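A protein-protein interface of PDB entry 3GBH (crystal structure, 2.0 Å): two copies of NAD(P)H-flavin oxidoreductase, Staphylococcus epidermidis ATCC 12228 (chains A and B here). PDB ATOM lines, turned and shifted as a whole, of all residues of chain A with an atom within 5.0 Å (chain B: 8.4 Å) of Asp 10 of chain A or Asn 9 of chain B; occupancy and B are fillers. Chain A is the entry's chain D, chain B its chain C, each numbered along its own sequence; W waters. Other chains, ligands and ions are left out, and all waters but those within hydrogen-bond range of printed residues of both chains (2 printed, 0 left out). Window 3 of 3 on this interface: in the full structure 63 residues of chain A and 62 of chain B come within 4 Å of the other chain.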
ATOM      1  N   ILE A   8      28.195 -22.874  -8.090  1.00  0.00           N
ATOM      2  CA  ILE A   8      27.566 -23.761  -7.127  1.00  0.00           C
ATOM      3  C   ILE A   8      26.045 -23.558  -7.227  1.00  0.00           C
ATOM      4  O   ILE A   8      25.546 -22.451  -6.993  1.00  0.00           O
ATOM      5  CB  ILE A   8      28.014 -23.486  -5.677  1.00  0.00           C
ATOM      6  CG1 ILE A   8      29.532 -23.505  -5.546  1.00  0.00           C
ATOM      7  CG2 ILE A   8      27.442 -24.563  -4.716  1.00  0.00           C
ATOM      8  CD1 ILE A   8      30.002 -23.224  -4.100  1.00  0.00           C
ATOM      9  N   ASN A   9      25.349 -24.629  -7.614  1.00  0.00           N
ATOM     10  CA  ASN A   9      23.893 -24.574  -7.808  1.00  0.00           C
ATOM     11  C   ASN A   9      23.068 -25.035  -6.606  1.00  0.00           C
ATOM     12  O   ASN A   9      21.911 -24.631  -6.455  1.00  0.00           O
ATOM     13  CB  ASN A   9      23.497 -25.405  -9.034  1.00  0.00           C
ATOM     14  CG  ASN A   9      24.091 -24.860 -10.323  1.00  0.00           C
ATOM     15  OD1 ASN A   9      23.928 -23.686 -10.643  1.00  0.00           O
ATOM     16  ND2 ASN A   9      24.777 -25.718 -11.071  1.00  0.00           N
ATOM     17  N   ASP A  10      23.639 -25.862  -5.745  1.00  0.00           N
ATOM     18  CA  ASP A  10      22.891 -26.411  -4.617  1.00  0.00           C
ATOM     19  C   ASP A  10      22.857 -25.447  -3.434  1.00  0.00           C
ATOM     20  O   ASP A  10      23.892 -24.985  -2.948  1.00  0.00           O
ATOM     21  CB  ASP A  10      23.493 -27.738  -4.188  1.00  0.00           C
ATOM     22  CG  ASP A  10      22.758 -28.340  -3.018  1.00  0.00           C
ATOM     23  OD1 ASP A  10      21.626 -28.837  -3.216  1.00  0.00           O
ATOM     24  OD2 ASP A  10      23.285 -28.283  -1.901  1.00  0.00           O
ATOM     25  N   PHE A  11      21.658 -25.165  -2.967  1.00  0.00           N
ATOM     26  CA  PHE A  11      21.450 -24.221  -1.881  1.00  0.00           C
ATOM     27  C   PHE A  11      22.316 -24.518  -0.654  1.00  0.00           C
ATOM     28  O   PHE A  11      23.036 -23.641  -0.185  1.00  0.00           O
ATOM     29  CB  PHE A  11      19.969 -24.173  -1.440  1.00  0.00           C
ATOM     30  CG  PHE A  11      19.736 -23.219  -0.309  1.00  0.00           C
ATOM     31  CD1 PHE A  11      19.696 -21.874  -0.551  1.00  0.00           C
ATOM     32  CD2 PHE A  11      19.639 -23.673   1.002  1.00  0.00           C
ATOM     33  CE1 PHE A  11      19.546 -20.952   0.507  1.00  0.00           C
ATOM     34  CE2 PHE A  11      19.474 -22.777   2.042  1.00  0.00           C
ATOM     35  CZ  PHE A  11      19.458 -21.419   1.803  1.00  0.00           C
ATOM     36  N   ASN A  12      22.242 -25.735  -0.130  1.00  0.00           N
ATOM     37  CA  ASN A  12      23.046 -26.104   1.045  1.00  0.00           C
ATOM     38  C   ASN A  12      24.544 -25.946   0.808  1.00  0.00           C
ATOM     39  O   ASN A  12      25.282 -25.524   1.699  1.00  0.00           O
ATOM     40  CB  ASN A  12      22.756 -27.539   1.490  1.00  0.00           C
ATOM     41  CG  ASN A  12      21.542 -27.634   2.359  1.00  0.00           C
ATOM     42  OD1 ASN A  12      21.182 -26.695   3.073  1.00  0.00           O
ATOM     43  ND2 ASN A  12      20.886 -28.779   2.307  1.00  0.00           N
ATOM     44  N   GLU A  13      24.990 -26.264  -0.399  1.00  0.00           N
ATOM     45  CA  GLU A  13      26.396 -26.165  -0.706  1.00  0.00           C
ATOM     46  C   GLU A  13      26.840 -24.700  -0.789  1.00  0.00           C
ATOM     47  O   GLU A  13      27.941 -24.382  -0.388  1.00  0.00           O
ATOM     48  CB  GLU A  13      26.740 -26.950  -1.989  1.00  0.00           C
ATOM     49  CG  GLU A  13      28.226 -27.001  -2.215  1.00  0.00           C
ATOM     50  CD  GLU A  13      28.657 -27.887  -3.398  1.00  0.00           C
ATOM     51  OE1 GLU A  13      27.777 -28.513  -4.064  1.00  0.00           O
ATOM     52  OE2 GLU A  13      29.895 -27.911  -3.639  1.00  0.00           O
ATOM     53  N   VAL A  14      25.968 -23.807  -1.234  1.00  0.00           N
ATOM     54  CA  VAL A  14      26.273 -22.382  -1.243  1.00  0.00           C
ATOM     55  C   VAL A  14      26.398 -21.869   0.191  1.00  0.00           C
ATOM     56  O   VAL A  14      27.389 -21.264   0.550  1.00  0.00           O
ATOM     57  CB  VAL A  14      25.212 -21.575  -2.040  1.00  0.00           C
ATOM     58  CG1 VAL A  14      25.472 -20.065  -1.985  1.00  0.00           C
ATOM     59  CG2 VAL A  14      25.142 -22.044  -3.472  1.00  0.00           C
ATOM     60  N   THR B   6       7.126 -29.477  -0.095  1.00  0.00           N
ATOM     61  CA  THR B   6       8.037 -29.521  -1.232  1.00  0.00           C
ATOM     62  C   THR B   6       9.223 -28.584  -0.992  1.00  0.00           C
ATOM     63  O   THR B   6       9.063 -27.379  -0.803  1.00  0.00           O
ATOM     64  CB  THR B   6       7.316 -29.167  -2.550  1.00  0.00           C
ATOM     65  OG1 THR B   6       6.244 -30.102  -2.759  1.00  0.00           O
ATOM     66  CG2 THR B   6       8.278 -29.251  -3.735  1.00  0.00           C
ATOM     67  N   ARG B   7      10.407 -29.176  -0.993  1.00  0.00           N
ATOM     68  CA  ARG B   7      11.652 -28.461  -0.803  1.00  0.00           C
ATOM     69  C   ARG B   7      12.159 -27.915  -2.102  1.00  0.00           C
ATOM     70  O   ARG B   7      11.732 -28.330  -3.166  1.00  0.00           O
ATOM     71  CB  ARG B   7      12.682 -29.405  -0.228  1.00  0.00           C
ATOM     72  CG  ARG B   7      12.209 -30.001   1.102  1.00  0.00           C
ATOM     73  CD  ARG B   7      13.360 -30.089   2.058  1.00  0.00           C
ATOM     74  NE  ARG B   7      12.972 -30.583   3.370  1.00  0.00           N
ATOM     75  CZ  ARG B   7      13.822 -30.689   4.384  1.00  0.00           C
ATOM     76  NH1 ARG B   7      15.089 -30.346   4.217  1.00  0.00           N
ATOM     77  NH2 ARG B   7      13.409 -31.142   5.556  1.00  0.00           N
ATOM     78  N   ILE B   8      13.054 -26.952  -1.998  1.00  0.00           N
ATOM     79  CA  ILE B   8      13.671 -26.299  -3.148  1.00  0.00           C
ATOM     80  C   ILE B   8      15.178 -26.399  -2.926  1.00  0.00           C
ATOM     81  O   ILE B   8      15.704 -25.823  -1.979  1.00  0.00           O
ATOM     82  CB  ILE B   8      13.255 -24.839  -3.254  1.00  0.00           C
ATOM     83  CG1 ILE B   8      11.745 -24.698  -3.294  1.00  0.00           C
ATOM     84  CG2 ILE B   8      13.806 -24.182  -4.555  1.00  0.00           C
ATOM     85  CD1 ILE B   8      11.298 -23.249  -3.525  1.00  0.00           C
ATOM     86  N   ASN B   9      15.850 -27.162  -3.775  1.00  0.00           N
ATOM     87  CA  ASN B   9      17.288 -27.453  -3.647  1.00  0.00           C
ATOM     88  C   ASN B   9      18.196 -26.497  -4.428  1.00  0.00           C
ATOM     89  O   ASN B   9      19.393 -26.372  -4.139  1.00  0.00           O
ATOM     90  CB  ASN B   9      17.564 -28.864  -4.167  1.00  0.00           C
ATOM     91  CG  ASN B   9      16.839 -29.950  -3.365  1.00  0.00           C
ATOM     92  OD1 ASN B   9      16.598 -29.799  -2.166  1.00  0.00           O
ATOM     93  ND2 ASN B   9      16.477 -31.034  -4.038  1.00  0.00           N
ATOM     94  N   ASP B  10      17.635 -25.869  -5.448  1.00  0.00           N
ATOM     95  CA  ASP B  10      18.401 -24.999  -6.309  1.00  0.00           C
ATOM     96  C   ASP B  10      18.500 -23.589  -5.725  1.00  0.00           C
ATOM     97  O   ASP B  10      17.489 -22.917  -5.504  1.00  0.00           O
ATOM     98  CB  ASP B  10      17.754 -24.958  -7.682  1.00  0.00           C
ATOM     99  CG  ASP B  10      18.468 -24.013  -8.632  1.00  0.00           C
ATOM    100  OD1 ASP B  10      19.553 -24.404  -9.166  1.00  0.00           O
ATOM    101  OD2 ASP B  10      17.952 -22.885  -8.849  1.00  0.00           O
ATOM    102  N   PHE B  11      19.733 -23.133  -5.515  1.00  0.00           N
ATOM    103  CA  PHE B  11      19.984 -21.802  -4.934  1.00  0.00           C
ATOM    104  C   PHE B  11      19.258 -20.635  -5.593  1.00  0.00           C
ATOM    105  O   PHE B  11      18.680 -19.802  -4.906  1.00  0.00           O
ATOM    106  CB  PHE B  11      21.472 -21.437  -4.939  1.00  0.00           C
ATOM    107  CG  PHE B  11      21.727 -20.062  -4.380  1.00  0.00           C
ATOM    108  CD1 PHE B  11      21.823 -19.873  -3.033  1.00  0.00           C
ATOM    109  CD2 PHE B  11      21.830 -18.960  -5.224  1.00  0.00           C
ATOM    110  CE1 PHE B  11      22.006 -18.597  -2.515  1.00  0.00           C
ATOM    111  CE2 PHE B  11      22.019 -17.683  -4.705  1.00  0.00           C
ATOM    112  CZ  PHE B  11      22.111 -17.508  -3.366  1.00  0.00           C
ATOM    113  N   ASN B  12      19.337 -20.523  -6.908  1.00  0.00           N
ATOM    114  CA  ASN B  12      18.679 -19.441  -7.612  1.00  0.00           C
ATOM    115  C   ASN B  12      17.166 -19.482  -7.422  1.00  0.00           C
ATOM    116  O   ASN B  12      16.516 -18.444  -7.271  1.00  0.00           O
ATOM    117  CB  ASN B  12      19.003 -19.472  -9.111  1.00  0.00           C
ATOM    118  CG  ASN B  12      18.683 -18.158  -9.796  1.00  0.00           C
ATOM    119  OD1 ASN B  12      19.092 -17.100  -9.325  1.00  0.00           O
ATOM    120  ND2 ASN B  12      17.942 -18.218 -10.909  1.00  0.00           N
ATOM    121  N   GLU B  13      16.598 -20.690  -7.443  1.00  0.00           N
ATOM    122  CA  GLU B  13      15.160 -20.808  -7.273  1.00  0.00           C
ATOM    123  C   GLU B  13      14.734 -20.412  -5.869  1.00  0.00           C
ATOM    124  O   GLU B  13      13.720 -19.774  -5.708  1.00  0.00           O
ATOM    125  CB  GLU B  13      14.656 -22.216  -7.582  1.00  0.00           C
ATOM    126  CG  GLU B  13      13.133 -22.295  -7.553  1.00  0.00           C
ATOM    127  CD  GLU B  13      12.559 -23.553  -8.207  1.00  0.00           C
ATOM    128  OE1 GLU B  13      13.331 -24.484  -8.523  1.00  0.00           O
ATOM    129  OE2 GLU B  13      11.325 -23.611  -8.372  1.00  0.00           O
ATOM    130  N   VAL B  14      15.506 -20.793  -4.857  1.00  0.00           N
ATOM    131  CA  VAL B  14      15.249 -20.357  -3.493  1.00  0.00           C
ATOM    132  C   VAL B  14      15.196 -18.830  -3.385  1.00  0.00           C
ATOM    133  O   VAL B  14      14.229 -18.244  -2.857  1.00  0.00           O
ATOM    134  CB  VAL B  14      16.284 -20.942  -2.493  1.00  0.00           C
ATOM    135  CG1 VAL B  14      16.118 -20.313  -1.107  1.00  0.00           C
ATOM    136  CG2 VAL B  14      16.172 -22.473  -2.425  1.00  0.00           C
ATOM    137  N   LYS B 155      12.738 -21.015   3.192  1.00  0.00           N
ATOM    138  CA  LYS B 155      12.207 -21.251   1.847  1.00  0.00           C
ATOM    139  C   LYS B 155      12.760 -22.549   1.236  1.00  0.00           C
ATOM    140  O   LYS B 155      11.989 -23.374   0.685  1.00  0.00           O
ATOM    141  CB  LYS B 155      12.458 -20.044   0.950  1.00  0.00           C
ATOM    142  CG  LYS B 155      11.896 -20.195  -0.434  1.00  0.00           C
ATOM    143  CD  LYS B 155      10.428 -19.909  -0.477  1.00  0.00           C
ATOM    144  CE  LYS B 155       9.610 -21.108  -0.614  1.00  0.00           C
ATOM    145  NZ  LYS B 155       8.246 -20.599  -0.854  1.00  0.00           N
ATOM    146  N   ALA B 156      14.065 -22.791   1.390  1.00  0.00           N
ATOM    147  CA  ALA B 156      14.644 -24.059   0.918  1.00  0.00           C
ATOM    148  C   ALA B 156      13.912 -25.241   1.532  1.00  0.00           C
ATOM    149  O   ALA B 156      13.741 -26.293   0.896  1.00  0.00           O
ATOM    150  CB  ALA B 156      16.154 -24.131   1.225  1.00  0.00           C
ATOM    151  N   HIS B 157      13.457 -25.079   2.767  1.00  0.00           N
ATOM    152  CA  HIS B 157      12.662 -26.118   3.428  1.00  0.00           C
ATOM    153  C   HIS B 157      11.187 -26.180   3.046  1.00  0.00           C
ATOM    154  O   HIS B 157      10.457 -27.058   3.546  1.00  0.00           O
ATOM    155  CB  HIS B 157      12.794 -25.993   4.946  1.00  0.00           C
ATOM    156  CG  HIS B 157      14.080 -26.537   5.490  1.00  0.00           C
ATOM    157  ND1 HIS B 157      14.118 -27.581   6.394  1.00  0.00           N
ATOM    158  CD2 HIS B 157      15.366 -26.163   5.282  1.00  0.00           C
ATOM    159  CE1 HIS B 157      15.377 -27.821   6.714  1.00  0.00           C
ATOM    160  NE2 HIS B 157      16.153 -26.973   6.055  1.00  0.00           N
ATOM    161  N   GLY B 158      10.721 -25.276   2.186  1.00  0.00           N
ATOM    162  CA  GLY B 158       9.317 -25.294   1.757  1.00  0.00           C
ATOM    163  C   GLY B 158       8.396 -24.384   2.573  1.00  0.00           C
ATOM    164  O   GLY B 158       7.184 -24.327   2.331  1.00  0.00           O
HETATM  165  O   HOH W   1      20.250 -27.757  -1.082  1.00  0.00           O
HETATM  166  O   HOH W   2      21.251 -22.189  -8.544  1.00  0.00           O
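O of Asn 9 of chain B sits at hydrogen-bond distance from N of Phe 11 of chain A (2.8 Å).
The backbone NH (N) of Phe 11 of chain B sits at hydrogen-bond distance from the backbone carbonyl oxygen (O) of Asn 9 of chain A (2.8 Å).
O of Asn 9 of chain B sits close to OD1 of Asp 10 of chain A (3.5 Å).
Water W1 lies within hydrogen-bond range of the side-chain carboxylate (OD1) of Asp 10 of chain A, the backbone NH (N) of Asn 12 of chain A and the backbone carbonyl oxygen (O) of Asn 9 of chain B.
Water W2 lies within hydrogen-bond range of OD1 of Asp 10 of chain B, N of Asn 12 of chain B and O of Asn 9 of chain A.
The backbone NH of Glu 13 of chain A sits at hydrogen-bond distance from the side-chain carboxylate of Asp 10 of chain A (3.0 Å).
The side-chain carboxylate of Asp 10 of chain A lies within hydrogen-bond range of the backbone NH of Asn 12 of chain A (3.3 Å).
OD2 of Asp 10 of chain B sits at hydrogen-bond distance from N of Glu 13 of chain B (2.9 Å).
The side-chain carboxylate of Asp 10 of chain B lies within hydrogen-bond range of the backbone NH of Asn 12 of chain B (3.4 Å).
The backbone NH of Ile 8 of chain B is in hydrogen-bond range of the backbone carbonyl oxygen of Ala 156 of chain B (3.0 Å).
Of the 13 printed residues of chain B, 5 touch a printed residue of chain A.
Hydrophobic or aromatic side chains of chain B within 4 Å of the printed part of chain A: Phe 11, Val 14 and Ala 156.
Along chain B the printed residues that touch a printed residue of chain A span positions 9 to 156.
Of the 7 printed residues of chain A, 4 touch a printed residue of chain B.
Among the printed residues, no Asp or Glu carboxylate lies within 4 Å of a Lys or Arg side-chain nitrogen of the other chain.
Asn 9 of chain B touches Asn 9 of chain A (O to O, 3.8 Å).
CA of Asp 10 of chain B touches O of Asn 9 of chain A, at 3.5 Å.
N of Phe 11 of chain A touches N of Phe 11 of chain B, at 3.8 Å.
CG1 of Val 14 of chain B touches CE1 of Phe 11 of chain A, at 3.8 Å.
Phe 11 of chain A touches Ala 156 of chain B (CD2 to CB, 3.5 Å).
CG1 of Val 14 of chain A touches CE1 of Phe 11 of chain B, 3.8 Å away.
Asn 9 of chain A touches its own counterpart, Asn 9 of chain B.
Asn 9 of chain A touches Phe 11 of chain B, and with the chains exchanged Phe 11 of chain A touches Asn 9 of chain B.
Phe 11 of chain A touches its own counterpart, Phe 11 of chain B.
Phe 11 of chain A touches Val 14 of chain B, and with the chains exchanged Val 14 of chain A touches Phe 11 of chain B.
7 positions are printed for both chains.
Asp 10 of chain A touches just one residue of chain B: Asn 9.
Of the printed residues of chain A, Asn 9 of chain B touches Asn 9 (3.8 Å), Asp 10 (3.5 Å) and Phe 11 (2.8 Å).
Printed residues of chain A within 4 Å of Phe 11 of chain B: Asn 9, Phe 11 and Val 14.
Of the printed residues of chain B, Asn 9 of chain A touches Asn 9 (3.8 Å), Asp 10 (3.5 Å) and Phe 11 (2.8 Å).
Of the printed residues of chain A, Ala 156 of chain B touches Phe 11 (3.5 Å).
Printed residues of chain A within 4 Å of Asp 10 of chain B: Asn 9.
Gly 158 of chain B touches none of the printed residues of chain A.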
